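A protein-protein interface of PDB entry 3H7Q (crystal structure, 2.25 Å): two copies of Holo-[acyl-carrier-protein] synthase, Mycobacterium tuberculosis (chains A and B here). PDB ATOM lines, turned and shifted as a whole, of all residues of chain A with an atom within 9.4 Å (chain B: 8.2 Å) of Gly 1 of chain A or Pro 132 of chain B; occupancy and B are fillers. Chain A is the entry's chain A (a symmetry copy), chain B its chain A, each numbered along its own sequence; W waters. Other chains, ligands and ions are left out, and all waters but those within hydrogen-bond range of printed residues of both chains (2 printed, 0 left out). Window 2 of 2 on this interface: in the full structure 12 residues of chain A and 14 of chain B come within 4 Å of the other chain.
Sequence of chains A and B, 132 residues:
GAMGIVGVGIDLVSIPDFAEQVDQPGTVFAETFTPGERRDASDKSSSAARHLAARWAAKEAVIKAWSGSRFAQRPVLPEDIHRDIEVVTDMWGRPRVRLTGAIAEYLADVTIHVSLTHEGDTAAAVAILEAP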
ATOM      1  N   GLY A   1     -20.345 -18.325   6.170  1.00  0.00           N
ATOM      2  CA  GLY A   1     -19.266 -17.455   5.738  1.00  0.00           C
ATOM      3  C   GLY A   1     -17.964 -17.752   6.460  1.00  0.00           C
ATOM      4  O   GLY A   1     -17.807 -18.816   7.049  1.00  0.00           O
ATOM      5  N   ALA A   2     -17.033 -16.806   6.409  1.00  0.00           N
ATOM      6  CA  ALA A   2     -15.739 -16.964   7.057  1.00  0.00           C
ATOM      7  C   ALA A   2     -15.852 -16.672   8.546  1.00  0.00           C
ATOM      8  O   ALA A   2     -16.153 -15.548   8.953  1.00  0.00           O
ATOM      9  CB  ALA A   2     -14.702 -16.057   6.409  1.00  0.00           C
ATOM     10  N   MET A   3     -15.601 -17.691   9.358  1.00  0.00           N
ATOM     11  CA  MET A   3     -15.799 -17.571  10.790  1.00  0.00           C
ATOM     12  C   MET A   3     -14.645 -18.157  11.590  1.00  0.00           C
ATOM     13  O   MET A   3     -13.901 -19.004  11.107  1.00  0.00           O
ATOM     14  CB  MET A   3     -17.114 -18.241  11.180  1.00  0.00           C
ATOM     15  CG  MET A   3     -18.327 -17.617  10.503  1.00  0.00           C
ATOM     16  SD  MET A   3     -18.930 -16.167  11.380  1.00  0.00           S
ATOM     17  CE  MET A   3     -20.134 -16.921  12.456  1.00  0.00           C
ATOM     18  N   GLY A   4     -14.492 -17.671  12.814  1.00  0.00           N
ATOM     19  CA  GLY A   4     -13.526 -18.216  13.741  1.00  0.00           C
ATOM     20  C   GLY A   4     -14.241 -18.647  15.008  1.00  0.00           C
ATOM     21  O   GLY A   4     -15.247 -18.045  15.399  1.00  0.00           O
ATOM     22  N   THR A 111     -22.242 -15.796  17.159  1.00  0.00           N
ATOM     23  CA  THR A 111     -23.207 -16.836  16.825  1.00  0.00           C
ATOM     24  C   THR A 111     -23.064 -18.013  17.774  1.00  0.00           C
ATOM     25  O   THR A 111     -21.963 -18.518  17.988  1.00  0.00           O
ATOM     26  CB  THR A 111     -23.050 -17.317  15.380  1.00  0.00           C
ATOM     27  OG1 THR A 111     -23.152 -16.195  14.489  1.00  0.00           O
ATOM     28  CG2 THR A 111     -24.128 -18.341  15.046  1.00  0.00           C
ATOM     29  N   GLU A 130     -18.978 -18.532  17.999  1.00  0.00           N
ATOM     30  CA  GLU A 130     -18.391 -18.285  16.679  1.00  0.00           C
ATOM     31  C   GLU A 130     -18.525 -16.800  16.306  1.00  0.00           C
ATOM     32  O   GLU A 130     -19.527 -16.164  16.627  1.00  0.00           O
ATOM     33  CB  GLU A 130     -19.120 -19.147  15.636  1.00  0.00           C
ATOM     34  CG  GLU A 130     -18.285 -19.584  14.448  1.00  0.00           C
ATOM     35  CD  GLU A 130     -19.089 -20.349  13.392  1.00  0.00           C
ATOM     36  OE1 GLU A 130     -20.314 -20.146  13.283  1.00  0.00           O
ATOM     37  OE2 GLU A 130     -18.492 -21.149  12.650  1.00  0.00           O
ATOM     38  N   ALA A 131     -17.525 -16.254  15.620  1.00  0.00           N
ATOM     39  CA  ALA A 131     -17.556 -14.852  15.187  1.00  0.00           C
ATOM     40  C   ALA A 131     -16.610 -14.596  14.014  1.00  0.00           C
ATOM     41  O   ALA A 131     -15.564 -15.233  13.903  1.00  0.00           O
ATOM     42  CB  ALA A 131     -17.217 -13.925  16.350  1.00  0.00           C
ATOM     43  N   PRO A 132     -16.976 -13.655  13.131  1.00  0.00           N
ATOM     44  CA  PRO A 132     -16.149 -13.342  11.956  1.00  0.00           C
ATOM     45  C   PRO A 132     -14.772 -12.812  12.346  1.00  0.00           C
ATOM     46  O   PRO A 132     -14.518 -12.482  13.503  1.00  0.00           O
ATOM     47  CB  PRO A 132     -16.954 -12.238  11.250  1.00  0.00           C
ATOM     48  CG  PRO A 132     -17.835 -11.669  12.340  1.00  0.00           C
ATOM     49  CD  PRO A 132     -18.225 -12.877  13.128  1.00  0.00           C
ATOM     50  OXT PRO A 132     -13.876 -12.700  11.509  1.00  0.00           O
ATOM     51  N   GLY B   1      -9.503 -23.683   5.184  1.00  0.00           N
ATOM     52  CA  GLY B   1      -9.867 -22.407   4.594  1.00  0.00           C
ATOM     53  C   GLY B   1     -10.893 -21.660   5.427  1.00  0.00           C
ATOM     54  O   GLY B   1     -11.085 -21.965   6.599  1.00  0.00           O
ATOM     55  N   ALA B   2     -11.550 -20.680   4.815  1.00  0.00           N
ATOM     56  CA  ALA B   2     -12.557 -19.885   5.500  1.00  0.00           C
ATOM     57  C   ALA B   2     -13.879 -20.637   5.557  1.00  0.00           C
ATOM     58  O   ALA B   2     -14.497 -20.916   4.527  1.00  0.00           O
ATOM     59  CB  ALA B   2     -12.735 -18.539   4.812  1.00  0.00           C
ATOM     60  N   MET B   3     -14.313 -20.958   6.769  1.00  0.00           N
ATOM     61  CA  MET B   3     -15.492 -21.784   6.946  1.00  0.00           C
ATOM     62  C   MET B   3     -16.425 -21.248   8.020  1.00  0.00           C
ATOM     63  O   MET B   3     -16.014 -20.505   8.907  1.00  0.00           O
ATOM     64  CB  MET B   3     -15.068 -23.214   7.271  1.00  0.00           C
ATOM     65  CG  MET B   3     -14.230 -23.853   6.173  1.00  0.00           C
ATOM     66  SD  MET B   3     -15.241 -24.565   4.866  1.00  0.00           S
ATOM     67  CE  MET B   3     -15.415 -26.233   5.467  1.00  0.00           C
ATOM     68  N   GLY B   4     -17.695 -21.614   7.913  1.00  0.00           N
ATOM     69  CA  GLY B   4     -18.675 -21.294   8.926  1.00  0.00           C
ATOM     70  C   GLY B   4     -19.317 -22.577   9.419  1.00  0.00           C
ATOM     71  O   GLY B   4     -19.460 -23.541   8.661  1.00  0.00           O
ATOM     72  N   ILE B   5     -19.692 -22.601  10.693  1.00  0.00           N
ATOM     73  CA  ILE B   5     -20.361 -23.765  11.250  1.00  0.00           C
ATOM     74  C   ILE B   5     -21.832 -23.760  10.859  1.00  0.00           C
ATOM     75  O   ILE B   5     -22.512 -22.746  10.989  1.00  0.00           O
ATOM     76  CB  ILE B   5     -20.221 -23.821  12.786  1.00  0.00           C
ATOM     77  CG1 ILE B   5     -18.775 -24.133  13.169  1.00  0.00           C
ATOM     78  CG2 ILE B   5     -21.179 -24.862  13.384  1.00  0.00           C
ATOM     79  CD1 ILE B   5     -18.530 -24.098  14.663  1.00  0.00           C
ATOM     80  N   VAL B   6     -22.312 -24.905  10.391  1.00  0.00           N
ATOM     81  CA  VAL B   6     -23.672 -25.051   9.891  1.00  0.00           C
ATOM     82  C   VAL B   6     -24.621 -25.773  10.866  1.00  0.00           C
ATOM     83  O   VAL B   6     -25.837 -25.581  10.819  1.00  0.00           O
ATOM     84  CB  VAL B   6     -23.658 -25.769   8.519  1.00  0.00           C
ATOM     85  CG1 VAL B   6     -24.907 -26.603   8.315  1.00  0.00           C
ATOM     86  CG2 VAL B   6     -23.482 -24.757   7.394  1.00  0.00           C
ATOM     87  N   ARG B  70     -30.138 -25.629   7.990  1.00  0.00           N
ATOM     88  CA  ARG B  70     -30.923 -25.078   6.887  1.00  0.00           C
ATOM     89  C   ARG B  70     -31.256 -26.102   5.807  1.00  0.00           C
ATOM     90  O   ARG B  70     -31.722 -25.743   4.723  1.00  0.00           O
ATOM     91  CB  ARG B  70     -30.196 -23.896   6.250  1.00  0.00           C
ATOM     92  CG  ARG B  70     -28.768 -24.194   5.833  1.00  0.00           C
ATOM     93  CD  ARG B  70     -28.450 -23.574   4.483  1.00  0.00           C
ATOM     94  NE  ARG B  70     -27.016 -23.543   4.226  1.00  0.00           N
ATOM     95  CZ  ARG B  70     -26.466 -23.712   3.028  1.00  0.00           C
ATOM     96  NH1 ARG B  70     -27.229 -23.940   1.965  1.00  0.00           N
ATOM     97  NH2 ARG B  70     -25.148 -23.667   2.894  1.00  0.00           N
ATOM     98  N   ASP B 109     -21.745 -30.264  -0.574  1.00  0.00           N
ATOM     99  CA  ASP B 109     -20.724 -29.265  -0.286  1.00  0.00           C
ATOM    100  C   ASP B 109     -20.613 -28.909   1.204  1.00  0.00           C
ATOM    101  O   ASP B 109     -20.198 -27.809   1.557  1.00  0.00           O
ATOM    102  CB  ASP B 109     -20.953 -28.013  -1.138  1.00  0.00           C
ATOM    103  CG  ASP B 109     -20.596 -28.238  -2.605  1.00  0.00           C
ATOM    104  OD1 ASP B 109     -19.479 -27.858  -3.011  1.00  0.00           O
ATOM    105  OD2 ASP B 109     -21.419 -28.814  -3.348  1.00  0.00           O
ATOM    106  N   VAL B 110     -20.977 -29.847   2.071  1.00  0.00           N
ATOM    107  CA  VAL B 110     -20.867 -29.634   3.507  1.00  0.00           C
ATOM    108  C   VAL B 110     -19.855 -30.607   4.100  1.00  0.00           C
ATOM    109  O   VAL B 110     -19.869 -31.794   3.792  1.00  0.00           O
ATOM    110  CB  VAL B 110     -22.243 -29.773   4.219  1.00  0.00           C
ATOM    111  CG1 VAL B 110     -22.089 -29.653   5.726  1.00  0.00           C
ATOM    112  CG2 VAL B 110     -23.221 -28.722   3.708  1.00  0.00           C
ATOM    113  N   THR B 111     -18.964 -30.099   4.941  1.00  0.00           N
ATOM    114  CA  THR B 111     -17.936 -30.943   5.537  1.00  0.00           C
ATOM    115  C   THR B 111     -18.387 -31.447   6.896  1.00  0.00           C
ATOM    116  O   THR B 111     -18.830 -30.668   7.739  1.00  0.00           O
ATOM    117  CB  THR B 111     -16.603 -30.203   5.678  1.00  0.00           C
ATOM    118  OG1 THR B 111     -16.197 -29.699   4.396  1.00  0.00           O
ATOM    119  CG2 THR B 111     -15.534 -31.141   6.226  1.00  0.00           C
ATOM    120  N   GLU B 130     -20.018 -28.081   8.637  1.00  0.00           N
ATOM    121  CA  GLU B 130     -19.216 -26.913   8.263  1.00  0.00           C
ATOM    122  C   GLU B 130     -19.364 -26.624   6.760  1.00  0.00           C
ATOM    123  O   GLU B 130     -19.461 -27.547   5.955  1.00  0.00           O
ATOM    124  CB  GLU B 130     -17.741 -27.191   8.593  1.00  0.00           C
ATOM    125  CG  GLU B 130     -16.911 -25.974   8.956  1.00  0.00           C
ATOM    126  CD  GLU B 130     -15.428 -26.296   9.170  1.00  0.00           C
ATOM    127  OE1 GLU B 130     -14.921 -27.277   8.594  1.00  0.00           O
ATOM    128  OE2 GLU B 130     -14.757 -25.553   9.907  1.00  0.00           O
ATOM    129  N   ALA B 131     -19.369 -25.348   6.386  1.00  0.00           N
ATOM    130  CA  ALA B 131     -19.478 -24.954   4.976  1.00  0.00           C
ATOM    131  C   ALA B 131     -18.946 -23.542   4.736  1.00  0.00           C
ATOM    132  O   ALA B 131     -19.044 -22.679   5.607  1.00  0.00           O
ATOM    133  CB  ALA B 131     -20.922 -25.062   4.500  1.00  0.00           C
ATOM    134  N   PRO B 132     -18.379 -23.299   3.544  1.00  0.00           N
ATOM    135  CA  PRO B 132     -17.818 -21.980   3.215  1.00  0.00           C
ATOM    136  C   PRO B 132     -18.880 -20.884   3.226  1.00  0.00           C
ATOM    137  O   PRO B 132     -20.079 -21.156   3.275  1.00  0.00           O
ATOM    138  CB  PRO B 132     -17.284 -22.177   1.786  1.00  0.00           C
ATOM    139  CG  PRO B 132     -18.060 -23.366   1.264  1.00  0.00           C
ATOM    140  CD  PRO B 132     -18.152 -24.263   2.455  1.00  0.00           C
ATOM    141  OXT PRO B 132     -18.564 -19.695   3.185  1.00  0.00           O
HETATM  142  O   HOH W   1     -21.338 -21.435   6.058  1.00  0.00           O
HETATM  143  O   HOH W   2     -21.880 -20.023  10.959  1.00  0.00           O
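The backbone NH (N) of Gly 4 of chain B lies within hydrogen-bond range of the backbone carbonyl oxygen (O) of Gly 1 of chain A (2.9 Å). O of Met 3 of chain B is in hydrogen-bond range of N of Met 3 of chain A (2.9 Å). The backbone carbonyl oxygen of Gly 1 of chain A lies close to the backbone carbonyl oxygen of Met 3 of chain B, at 3.1 Å. OE2 of Glu 130 of chain A sits at hydrogen-bond distance from N of Ile 5 of chain B (2.7 Å).
O of Ala 131 of chain B lies within hydrogen-bond range of N of Gly 4 of chain B, 2.9 Å away. The backbone NH (N) of Thr 111 of chain A is in hydrogen-bond range of the backbone carbonyl oxygen (O) of Glu 130 of chain A (2.8 Å).
Among the printed residues, pairs that only touch across the chains: Gly 1 of chain A with Pro 132 of chain B (3.5 Å), Ala 2 of chain A with Ala 2 of chain B (3.5 Å), Glu 130 of chain A with Gly 4 of chain B (3.6 Å) and Ala 2 of chain A with Met 3 of chain B (3.9 Å).
Pro 132 of chain B touches just one residue of chain A: Gly 1. Ala 2 of chain A touches just these residues of chain B: Ala 2 and Met 3. No residue of chain A comes within 4 Å of Ala 131 of chain B. Printed residues of chain A within 4 Å of Gly 4 of chain B: Gly 1 and Glu 130. Printed residues of chain B within 4 Å of Glu 130 of chain A: Gly 4 (3.6 Å) and Ile 5 (2.7 Å). Of the printed residues of chain B, Met 3 of chain A touches Met 3 (2.9 Å). Printed residues of chain A within 4 Å of Ala 2 of chain B: Ala 2. Thr 111 of chain A touches none of the printed residues of chain B. Pro 132 of chain A touches none of the printed residues of chain B. The nearest residue of chain B that does not touch Gly 1 of chain A is Ala 131 of chain B (4.3 Å). The nearest printed residue of chain A that does not touch Ile 5 of chain B is Met 3 of chain A (5.1 Å).
Of the 8 printed residues of chain A, 4 touch a printed residue of chain B. Printed residues of chain A that touch a printed residue of chain B: Gly 1, Ala 2, Met 3 and Glu 130. Hydrophobic or aromatic side chains of chain A within 4 Å of the printed part of chain B: Ala 2 and Met 3. Along chain A the printed residues that touch a printed residue of chain B span positions 1 to 130. Hydrophobic or aromatic side chains of chain B that line the printed part of chain A: Ala 2 and Ile 5. Along chain B the printed residues that touch a printed residue of chain A span positions 2 to 132. Among the printed residues, 8 pairs touch across the chains. Among the printed residues, no Asp or Glu carboxylate lies within 4 Å of a Lys or Arg side-chain nitrogen of the other chain.
Gly 1 of chain A touches Met 3 of chain B, but with the chains exchanged Met 3 of chain A does not touch Gly 1 of chain B (6.1 Å). Gly 1 of chain A touches Gly 4 of chain B, but with the chains exchanged Gly 4 of chain A does not touch Gly 1 of chain B (8.3 Å). Gly 1 of chain A touches Pro 132 of chain B, but with the chains exchanged Pro 132 of chain A does not touch Gly 1 of chain B (10.9 Å). Ala 2 of chain A touches Met 3 of chain B, but with the chains exchanged Met 3 of chain A does not touch Ala 2 of chain B (5.1 Å). Positions printed for both chains: 1, 2, 3, 4, 111, 130, 131 and 132. Of the 8 pairs that touch across the chains among the printed residues, 2 have their exchanged pair printed and touching as well.
Water W1 lies within hydrogen-bond range of the backbone carbonyl oxygen of Ala 131 of chain B (2.6 Å), the chain-end carboxylate of Pro 132 of chain B (3.1 Å) and the backbone NH of Gly 1 of chain A (3.3 Å). Water W2 bridges the backbone carbonyl oxygen (O) of Ile 5 of chain B (2.8 Å) and the side-chain carboxylate (OE1) of Glu 130 of chain A (2.8 Å).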
